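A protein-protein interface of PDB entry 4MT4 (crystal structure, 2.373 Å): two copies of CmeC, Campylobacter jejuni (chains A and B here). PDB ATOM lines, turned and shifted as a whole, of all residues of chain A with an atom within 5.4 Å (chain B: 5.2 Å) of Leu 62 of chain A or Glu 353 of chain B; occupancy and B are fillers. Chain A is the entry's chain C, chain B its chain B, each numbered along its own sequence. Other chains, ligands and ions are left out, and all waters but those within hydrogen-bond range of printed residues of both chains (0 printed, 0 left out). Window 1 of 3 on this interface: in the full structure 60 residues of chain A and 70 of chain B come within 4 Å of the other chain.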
ATOM      1  N   ASN A  58      25.790 -23.310 -22.963  1.00  0.00           N
ATOM      2  CA  ASN A  58      25.119 -22.083 -22.549  1.00  0.00           C
ATOM      3  C   ASN A  58      25.559 -21.576 -21.179  1.00  0.00           C
ATOM      4  O   ASN A  58      25.553 -20.369 -20.930  1.00  0.00           O
ATOM      5  CB  ASN A  58      23.604 -22.290 -22.559  1.00  0.00           C
ATOM      6  CG  ASN A  58      23.067 -22.582 -23.946  1.00  0.00           C
ATOM      7  OD1 ASN A  58      22.935 -21.682 -24.775  1.00  0.00           O
ATOM      8  ND2 ASN A  58      22.756 -23.846 -24.206  1.00  0.00           N
ATOM      9  N   ASP A  59      25.935 -22.494 -20.294  1.00  0.00           N
ATOM     10  CA  ASP A  59      26.462 -22.111 -18.987  1.00  0.00           C
ATOM     11  C   ASP A  59      27.773 -21.354 -19.154  1.00  0.00           C
ATOM     12  O   ASP A  59      28.069 -20.423 -18.410  1.00  0.00           O
ATOM     13  CB  ASP A  59      26.669 -23.340 -18.101  1.00  0.00           C
ATOM     14  CG  ASP A  59      25.364 -23.907 -17.577  1.00  0.00           C
ATOM     15  OD1 ASP A  59      24.467 -23.113 -17.225  1.00  0.00           O
ATOM     16  OD2 ASP A  59      25.236 -25.149 -17.519  1.00  0.00           O
ATOM     17  N   LEU A  60      28.554 -21.760 -20.147  1.00  0.00           N
ATOM     18  CA  LEU A  60      29.808 -21.089 -20.465  1.00  0.00           C
ATOM     19  C   LEU A  60      29.538 -19.701 -21.038  1.00  0.00           C
ATOM     20  O   LEU A  60      30.284 -18.756 -20.779  1.00  0.00           O
ATOM     21  CB  LEU A  60      30.630 -21.927 -21.450  1.00  0.00           C
ATOM     22  CG  LEU A  60      32.031 -21.416 -21.791  1.00  0.00           C
ATOM     23  CD1 LEU A  60      32.867 -21.265 -20.531  1.00  0.00           C
ATOM     24  CD2 LEU A  60      32.710 -22.352 -22.779  1.00  0.00           C
ATOM     25  N   LYS A  61      28.463 -19.588 -21.813  1.00  0.00           N
ATOM     26  CA  LYS A  61      28.063 -18.308 -22.387  1.00  0.00           C
ATOM     27  C   LYS A  61      27.556 -17.360 -21.305  1.00  0.00           C
ATOM     28  O   LYS A  61      27.830 -16.161 -21.340  1.00  0.00           O
ATOM     29  CB  LYS A  61      26.987 -18.510 -23.454  1.00  0.00           C
ATOM     30  CG  LYS A  61      27.443 -19.342 -24.642  1.00  0.00           C
ATOM     31  CD  LYS A  61      26.321 -19.529 -25.653  1.00  0.00           C
ATOM     32  CE  LYS A  61      26.715 -20.520 -26.738  1.00  0.00           C
ATOM     33  NZ  LYS A  61      25.664 -20.641 -27.787  1.00  0.00           N
ATOM     34  N   LEU A  62      26.816 -17.908 -20.344  1.00  0.00           N
ATOM     35  CA  LEU A  62      26.303 -17.124 -19.227  1.00  0.00           C
ATOM     36  C   LEU A  62      27.440 -16.549 -18.391  1.00  0.00           C
ATOM     37  O   LEU A  62      27.399 -15.387 -17.990  1.00  0.00           O
ATOM     38  CB  LEU A  62      25.386 -17.974 -18.348  1.00  0.00           C
ATOM     39  CG  LEU A  62      24.003 -18.290 -18.921  1.00  0.00           C
ATOM     40  CD1 LEU A  62      23.228 -19.205 -17.984  1.00  0.00           C
ATOM     41  CD2 LEU A  62      23.234 -17.006 -19.178  1.00  0.00           C
ATOM     42  N   ALA A  63      28.455 -17.367 -18.137  1.00  0.00           N
ATOM     43  CA  ALA A  63      29.617 -16.927 -17.378  1.00  0.00           C
ATOM     44  C   ALA A  63      30.395 -15.858 -18.141  1.00  0.00           C
ATOM     45  O   ALA A  63      31.010 -14.979 -17.539  1.00  0.00           O
ATOM     46  CB  ALA A  63      30.516 -18.108 -17.052  1.00  0.00           C
ATOM     47  N   PHE A  64      30.363 -15.938 -19.469  1.00  0.00           N
ATOM     48  CA  PHE A  64      31.004 -14.938 -20.316  1.00  0.00           C
ATOM     49  C   PHE A  64      30.239 -13.624 -20.238  1.00  0.00           C
ATOM     50  O   PHE A  64      30.836 -12.548 -20.207  1.00  0.00           O
ATOM     51  CB  PHE A  64      31.083 -15.421 -21.770  1.00  0.00           C
ATOM     52  CG  PHE A  64      31.956 -14.563 -22.651  1.00  0.00           C
ATOM     53  CD1 PHE A  64      31.432 -13.464 -23.311  1.00  0.00           C
ATOM     54  CD2 PHE A  64      33.298 -14.863 -22.826  1.00  0.00           C
ATOM     55  CE1 PHE A  64      32.229 -12.676 -24.120  1.00  0.00           C
ATOM     56  CE2 PHE A  64      34.099 -14.080 -23.634  1.00  0.00           C
ATOM     57  CZ  PHE A  64      33.564 -12.985 -24.283  1.00  0.00           C
ATOM     58  N   ILE A  65      28.914 -13.725 -20.213  1.00  0.00           N
ATOM     59  CA  ILE A  65      28.049 -12.554 -20.130  1.00  0.00           C
ATOM     60  C   ILE A  65      28.168 -11.887 -18.762  1.00  0.00           C
ATOM     61  O   ILE A  65      28.220 -10.660 -18.665  1.00  0.00           O
ATOM     62  CB  ILE A  65      26.579 -12.925 -20.402  1.00  0.00           C
ATOM     63  CG1 ILE A  65      26.407 -13.367 -21.857  1.00  0.00           C
ATOM     64  CG2 ILE A  65      25.658 -11.757 -20.091  1.00  0.00           C
ATOM     65  CD1 ILE A  65      25.045 -13.950 -22.165  1.00  0.00           C
ATOM     66  N   HIS A  66      28.222 -12.704 -17.712  1.00  0.00           N
ATOM     67  CA  HIS A  66      28.409 -12.211 -16.348  1.00  0.00           C
ATOM     68  C   HIS A  66      29.685 -11.381 -16.245  1.00  0.00           C
ATOM     69  O   HIS A  66      29.735 -10.384 -15.526  1.00  0.00           O
ATOM     70  CB  HIS A  66      28.458 -13.373 -15.349  1.00  0.00           C
ATOM     71  CG  HIS A  66      27.173 -14.134 -15.236  1.00  0.00           C
ATOM     72  ND1 HIS A  66      25.959 -13.611 -15.627  1.00  0.00           N
ATOM     73  CD2 HIS A  66      26.914 -15.383 -14.780  1.00  0.00           C
ATOM     74  CE1 HIS A  66      25.008 -14.503 -15.415  1.00  0.00           C
ATOM     75  NE2 HIS A  66      25.561 -15.588 -14.901  1.00  0.00           N
ATOM     76  N   MET A  67      30.711 -11.795 -16.981  1.00  0.00           N
ATOM     77  CA  MET A  67      31.977 -11.074 -17.022  1.00  0.00           C
ATOM     78  C   MET A  67      31.820  -9.738 -17.744  1.00  0.00           C
ATOM     79  O   MET A  67      32.395  -8.728 -17.335  1.00  0.00           O
ATOM     80  CB  MET A  67      33.050 -11.929 -17.704  1.00  0.00           C
ATOM     81  CG  MET A  67      34.398 -11.246 -17.880  1.00  0.00           C
ATOM     82  SD  MET A  67      35.653 -12.377 -18.505  1.00  0.00           S
ATOM     83  CE  MET A  67      34.789 -13.123 -19.885  1.00  0.00           C
ATOM     84  N   GLN A  69      28.971  -8.082 -18.011  1.00  0.00           N
ATOM     85  CA  GLN A  69      28.119  -7.268 -17.151  1.00  0.00           C
ATOM     86  C   GLN A  69      28.943  -6.567 -16.076  1.00  0.00           C
ATOM     87  O   GLN A  69      28.694  -5.409 -15.742  1.00  0.00           O
ATOM     88  CB  GLN A  69      27.031  -8.129 -16.506  1.00  0.00           C
ATOM     89  CG  GLN A  69      25.981  -8.648 -17.480  1.00  0.00           C
ATOM     90  CD  GLN A  69      25.123  -9.751 -16.889  1.00  0.00           C
ATOM     91  OE1 GLN A  69      25.565 -10.497 -16.018  1.00  0.00           O
ATOM     92  NE2 GLN A  69      23.884  -9.855 -17.361  1.00  0.00           N
ATOM     93  N   LEU B 349      23.075  -6.750 -22.239  1.00  0.00           N
ATOM     94  CA  LEU B 349      23.663  -7.989 -21.745  1.00  0.00           C
ATOM     95  C   LEU B 349      22.641  -8.797 -20.948  1.00  0.00           C
ATOM     96  O   LEU B 349      22.679 -10.027 -20.943  1.00  0.00           O
ATOM     97  CB  LEU B 349      24.894  -7.692 -20.890  1.00  0.00           C
ATOM     98  CG  LEU B 349      26.103  -7.138 -21.649  1.00  0.00           C
ATOM     99  CD1 LEU B 349      27.140  -6.573 -20.692  1.00  0.00           C
ATOM    100  CD2 LEU B 349      26.715  -8.212 -22.535  1.00  0.00           C
ATOM    101  N   ASN B 350      21.730  -8.098 -20.277  1.00  0.00           N
ATOM    102  CA  ASN B 350      20.640  -8.753 -19.563  1.00  0.00           C
ATOM    103  C   ASN B 350      19.712  -9.456 -20.542  1.00  0.00           C
ATOM    104  O   ASN B 350      19.191 -10.533 -20.260  1.00  0.00           O
ATOM    105  CB  ASN B 350      19.849  -7.746 -18.726  1.00  0.00           C
ATOM    106  CG  ASN B 350      20.676  -7.129 -17.617  1.00  0.00           C
ATOM    107  OD1 ASN B 350      21.766  -7.603 -17.301  1.00  0.00           O
ATOM    108  ND2 ASN B 350      20.155  -6.068 -17.011  1.00  0.00           N
ATOM    109  N   LYS B 351      19.514  -8.833 -21.697  1.00  0.00           N
ATOM    110  CA  LYS B 351      18.728  -9.430 -22.766  1.00  0.00           C
ATOM    111  C   LYS B 351      19.429 -10.661 -23.329  1.00  0.00           C
ATOM    112  O   LYS B 351      18.793 -11.683 -23.590  1.00  0.00           O
ATOM    113  CB  LYS B 351      18.474  -8.415 -23.881  1.00  0.00           C
ATOM    114  CG  LYS B 351      17.758  -8.999 -25.082  1.00  0.00           C
ATOM    115  CD  LYS B 351      17.787  -8.051 -26.265  1.00  0.00           C
ATOM    116  CE  LYS B 351      17.224  -8.724 -27.506  1.00  0.00           C
ATOM    117  NZ  LYS B 351      17.270  -7.832 -28.697  1.00  0.00           N
ATOM    118  N   ASP B 352      20.742 -10.552 -23.519  1.00  0.00           N
ATOM    119  CA  ASP B 352      21.546 -11.669 -24.004  1.00  0.00           C
ATOM    120  C   ASP B 352      21.462 -12.851 -23.044  1.00  0.00           C
ATOM    121  O   ASP B 352      21.373 -14.002 -23.467  1.00  0.00           O
ATOM    122  CB  ASP B 352      23.007 -11.248 -24.190  1.00  0.00           C
ATOM    123  CG  ASP B 352      23.178 -10.171 -25.249  1.00  0.00           C
ATOM    124  OD1 ASP B 352      22.234  -9.950 -26.038  1.00  0.00           O
ATOM    125  OD2 ASP B 352      24.262  -9.552 -25.298  1.00  0.00           O
ATOM    126  N   GLU B 353      21.495 -12.555 -21.749  1.00  0.00           N
ATOM    127  CA  GLU B 353      21.388 -13.584 -20.721  1.00  0.00           C
ATOM    128  C   GLU B 353      20.039 -14.290 -20.807  1.00  0.00           C
ATOM    129  O   GLU B 353      19.951 -15.509 -20.661  1.00  0.00           O
ATOM    130  CB  GLU B 353      21.584 -12.974 -19.332  1.00  0.00           C
ATOM    131  CG  GLU B 353      21.458 -13.969 -18.191  1.00  0.00           C
ATOM    132  CD  GLU B 353      21.783 -13.358 -16.843  1.00  0.00           C
ATOM    133  OE1 GLU B 353      21.992 -12.128 -16.774  1.00  0.00           O
ATOM    134  OE2 GLU B 353      21.833 -14.113 -15.849  1.00  0.00           O
ATOM    135  N   ALA B 354      18.990 -13.515 -21.060  1.00  0.00           N
ATOM    136  CA  ALA B 354      17.648 -14.064 -21.193  1.00  0.00           C
ATOM    137  C   ALA B 354      17.523 -14.889 -22.471  1.00  0.00           C
ATOM    138  O   ALA B 354      16.732 -15.828 -22.537  1.00  0.00           O
ATOM    139  CB  ALA B 354      16.614 -12.951 -21.174  1.00  0.00           C
ATOM    140  N   PHE B 355      18.305 -14.527 -23.485  1.00  0.00           N
ATOM    141  CA  PHE B 355      18.324 -15.269 -24.740  1.00  0.00           C
ATOM    142  C   PHE B 355      19.015 -16.612 -24.539  1.00  0.00           C
ATOM    143  O   PHE B 355      18.555 -17.636 -25.038  1.00  0.00           O
ATOM    144  CB  PHE B 355      19.031 -14.472 -25.844  1.00  0.00           C
ATOM    145  CG  PHE B 355      18.795 -15.014 -27.231  1.00  0.00           C
ATOM    146  CD1 PHE B 355      19.521 -16.097 -27.702  1.00  0.00           C
ATOM    147  CD2 PHE B 355      17.847 -14.439 -28.064  1.00  0.00           C
ATOM    148  CE1 PHE B 355      19.303 -16.598 -28.973  1.00  0.00           C
ATOM    149  CE2 PHE B 355      17.629 -14.934 -29.337  1.00  0.00           C
ATOM    150  CZ  PHE B 355      18.358 -16.014 -29.791  1.00  0.00           C
ATOM    151  N   VAL B 356      20.128 -16.595 -23.811  1.00  0.00           N
ATOM    152  CA  VAL B 356      20.875 -17.812 -23.520  1.00  0.00           C
ATOM    153  C   VAL B 356      20.041 -18.749 -22.650  1.00  0.00           C
ATOM    154  O   VAL B 356      20.072 -19.968 -22.824  1.00  0.00           O
ATOM    155  CB  VAL B 356      22.218 -17.499 -22.827  1.00  0.00           C
ATOM    156  CG1 VAL B 356      22.917 -18.776 -22.405  1.00  0.00           C
ATOM    157  CG2 VAL B 356      23.110 -16.690 -23.752  1.00  0.00           C
ATOM    158  N   ASN B 357      19.289 -18.168 -21.719  1.00  0.00           N
ATOM    159  CA  ASN B 357      18.358 -18.934 -20.901  1.00  0.00           C
ATOM    160  C   ASN B 357      17.288 -19.592 -21.763  1.00  0.00           C
ATOM    161  O   ASN B 357      16.859 -20.713 -21.491  1.00  0.00           O
ATOM    162  CB  ASN B 357      17.703 -18.043 -19.842  1.00  0.00           C
ATOM    163  CG  ASN B 357      18.654 -17.675 -18.720  1.00  0.00           C
ATOM    164  OD1 ASN B 357      19.692 -18.313 -18.537  1.00  0.00           O
ATOM    165  ND2 ASN B 357      18.298 -16.651 -17.953  1.00  0.00           N
ATOM    166  N   TYR B 358      16.865 -18.887 -22.809  1.00  0.00           N
ATOM    167  CA  TYR B 358      15.874 -19.416 -23.740  1.00  0.00           C
ATOM    168  C   TYR B 358      16.427 -20.603 -24.518  1.00  0.00           C
ATOM    169  O   TYR B 358      15.768 -21.636 -24.640  1.00  0.00           O
ATOM    170  CB  TYR B 358      15.410 -18.328 -24.710  1.00  0.00           C
ATOM    171  CG  TYR B 358      14.466 -18.831 -25.783  1.00  0.00           C
ATOM    172  CD1 TYR B 358      13.104 -18.946 -25.538  1.00  0.00           C
ATOM    173  CD2 TYR B 358      14.939 -19.189 -27.039  1.00  0.00           C
ATOM    174  CE1 TYR B 358      12.240 -19.406 -26.514  1.00  0.00           C
ATOM    175  CE2 TYR B 358      14.084 -19.650 -28.020  1.00  0.00           C
ATOM    176  CZ  TYR B 358      12.736 -19.756 -27.753  1.00  0.00           C
ATOM    177  OH  TYR B 358      11.882 -20.215 -28.730  1.00  0.00           O
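OD1 of Asn 350 of chain B is in hydrogen-bond range of NE2 of Gln 69 of chain A. The side-chain carboxylate (OE1) of Glu 353 of chain B is in hydrogen-bond range of the side-chain amide nitrogen (NE2) of Gln 69 of chain A (3.0 Å).
ND1 of His 66 of chain A sits close to O of Leu 62 of chain A (3.3 Å). ND1 of His 66 of chain A is in hydrogen-bond range of OE1 of Gln 69 of chain A (3.2 Å). ND2 of Asn 357 of chain B lies close to O of Glu 353 of chain B (3.4 Å).
Among the printed residues, pairs that only touch across the chains: Asn 58 of chain A with Val 356 of chain B (3.4 Å), Leu 62 of chain A with Glu 353 of chain B (3.7 Å), Leu 62 of chain A with Val 356 of chain B (3.7 Å), Leu 62 of chain A with Asn 357 of chain B (3.7 Å), Ile 65 of chain A with Leu 349 of chain B (3.5 Å), Ile 65 of chain A with Asp 352 of chain B (3.8 Å), Ile 65 of chain A with Glu 353 of chain B (3.8 Å), Ile 65 of chain A with Val 356 of chain B (3.7 Å), His 66 of chain A with Glu 353 of chain B (3.2 Å) and Gln 69 of chain A with Leu 349 of chain B (3.6 Å).
Of the printed residues of chain B, Leu 62 of chain A touches Glu 353, Val 356 and Asn 357. Printed residues of chain A within 4 Å of Leu 349 of chain B: Ile 65 and Gln 69. Printed residues of chain A within 4 Å of Asn 350 of chain B: Gln 69 (3.1 Å). Of the printed residues of chain A, Asp 352 of chain B touches Ile 65 (3.8 Å). Glu 353 of chain B touches just these residues of chain A: Leu 62, Ile 65, His 66 and Gln 69. Printed residues of chain A within 4 Å of Val 356 of chain B: Asn 58 (3.4 Å), Leu 62 (3.7 Å) and Ile 65 (3.7 Å). Of the printed residues of chain A, Asn 357 of chain B touches Leu 62 (3.7 Å). The nearest printed residue of chain A that does not touch Glu 353 of chain B is Lys 61 of chain A (7.0 Å).
Of the 11 printed residues of chain A, 5 touch a printed residue of chain B. Printed residues of chain A that touch a printed residue of chain B: Asn 58, Leu 62, Ile 65, His 66 and Gln 69. Of the 10 printed residues of chain B, 6 touch a printed residue of chain A. Among the printed residues, 12 pairs touch across the chains.
No position is printed for both chains. Of the 12 pairs that touch across the chains among the printed residues, none has its exchanged pair printed and touching as well.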
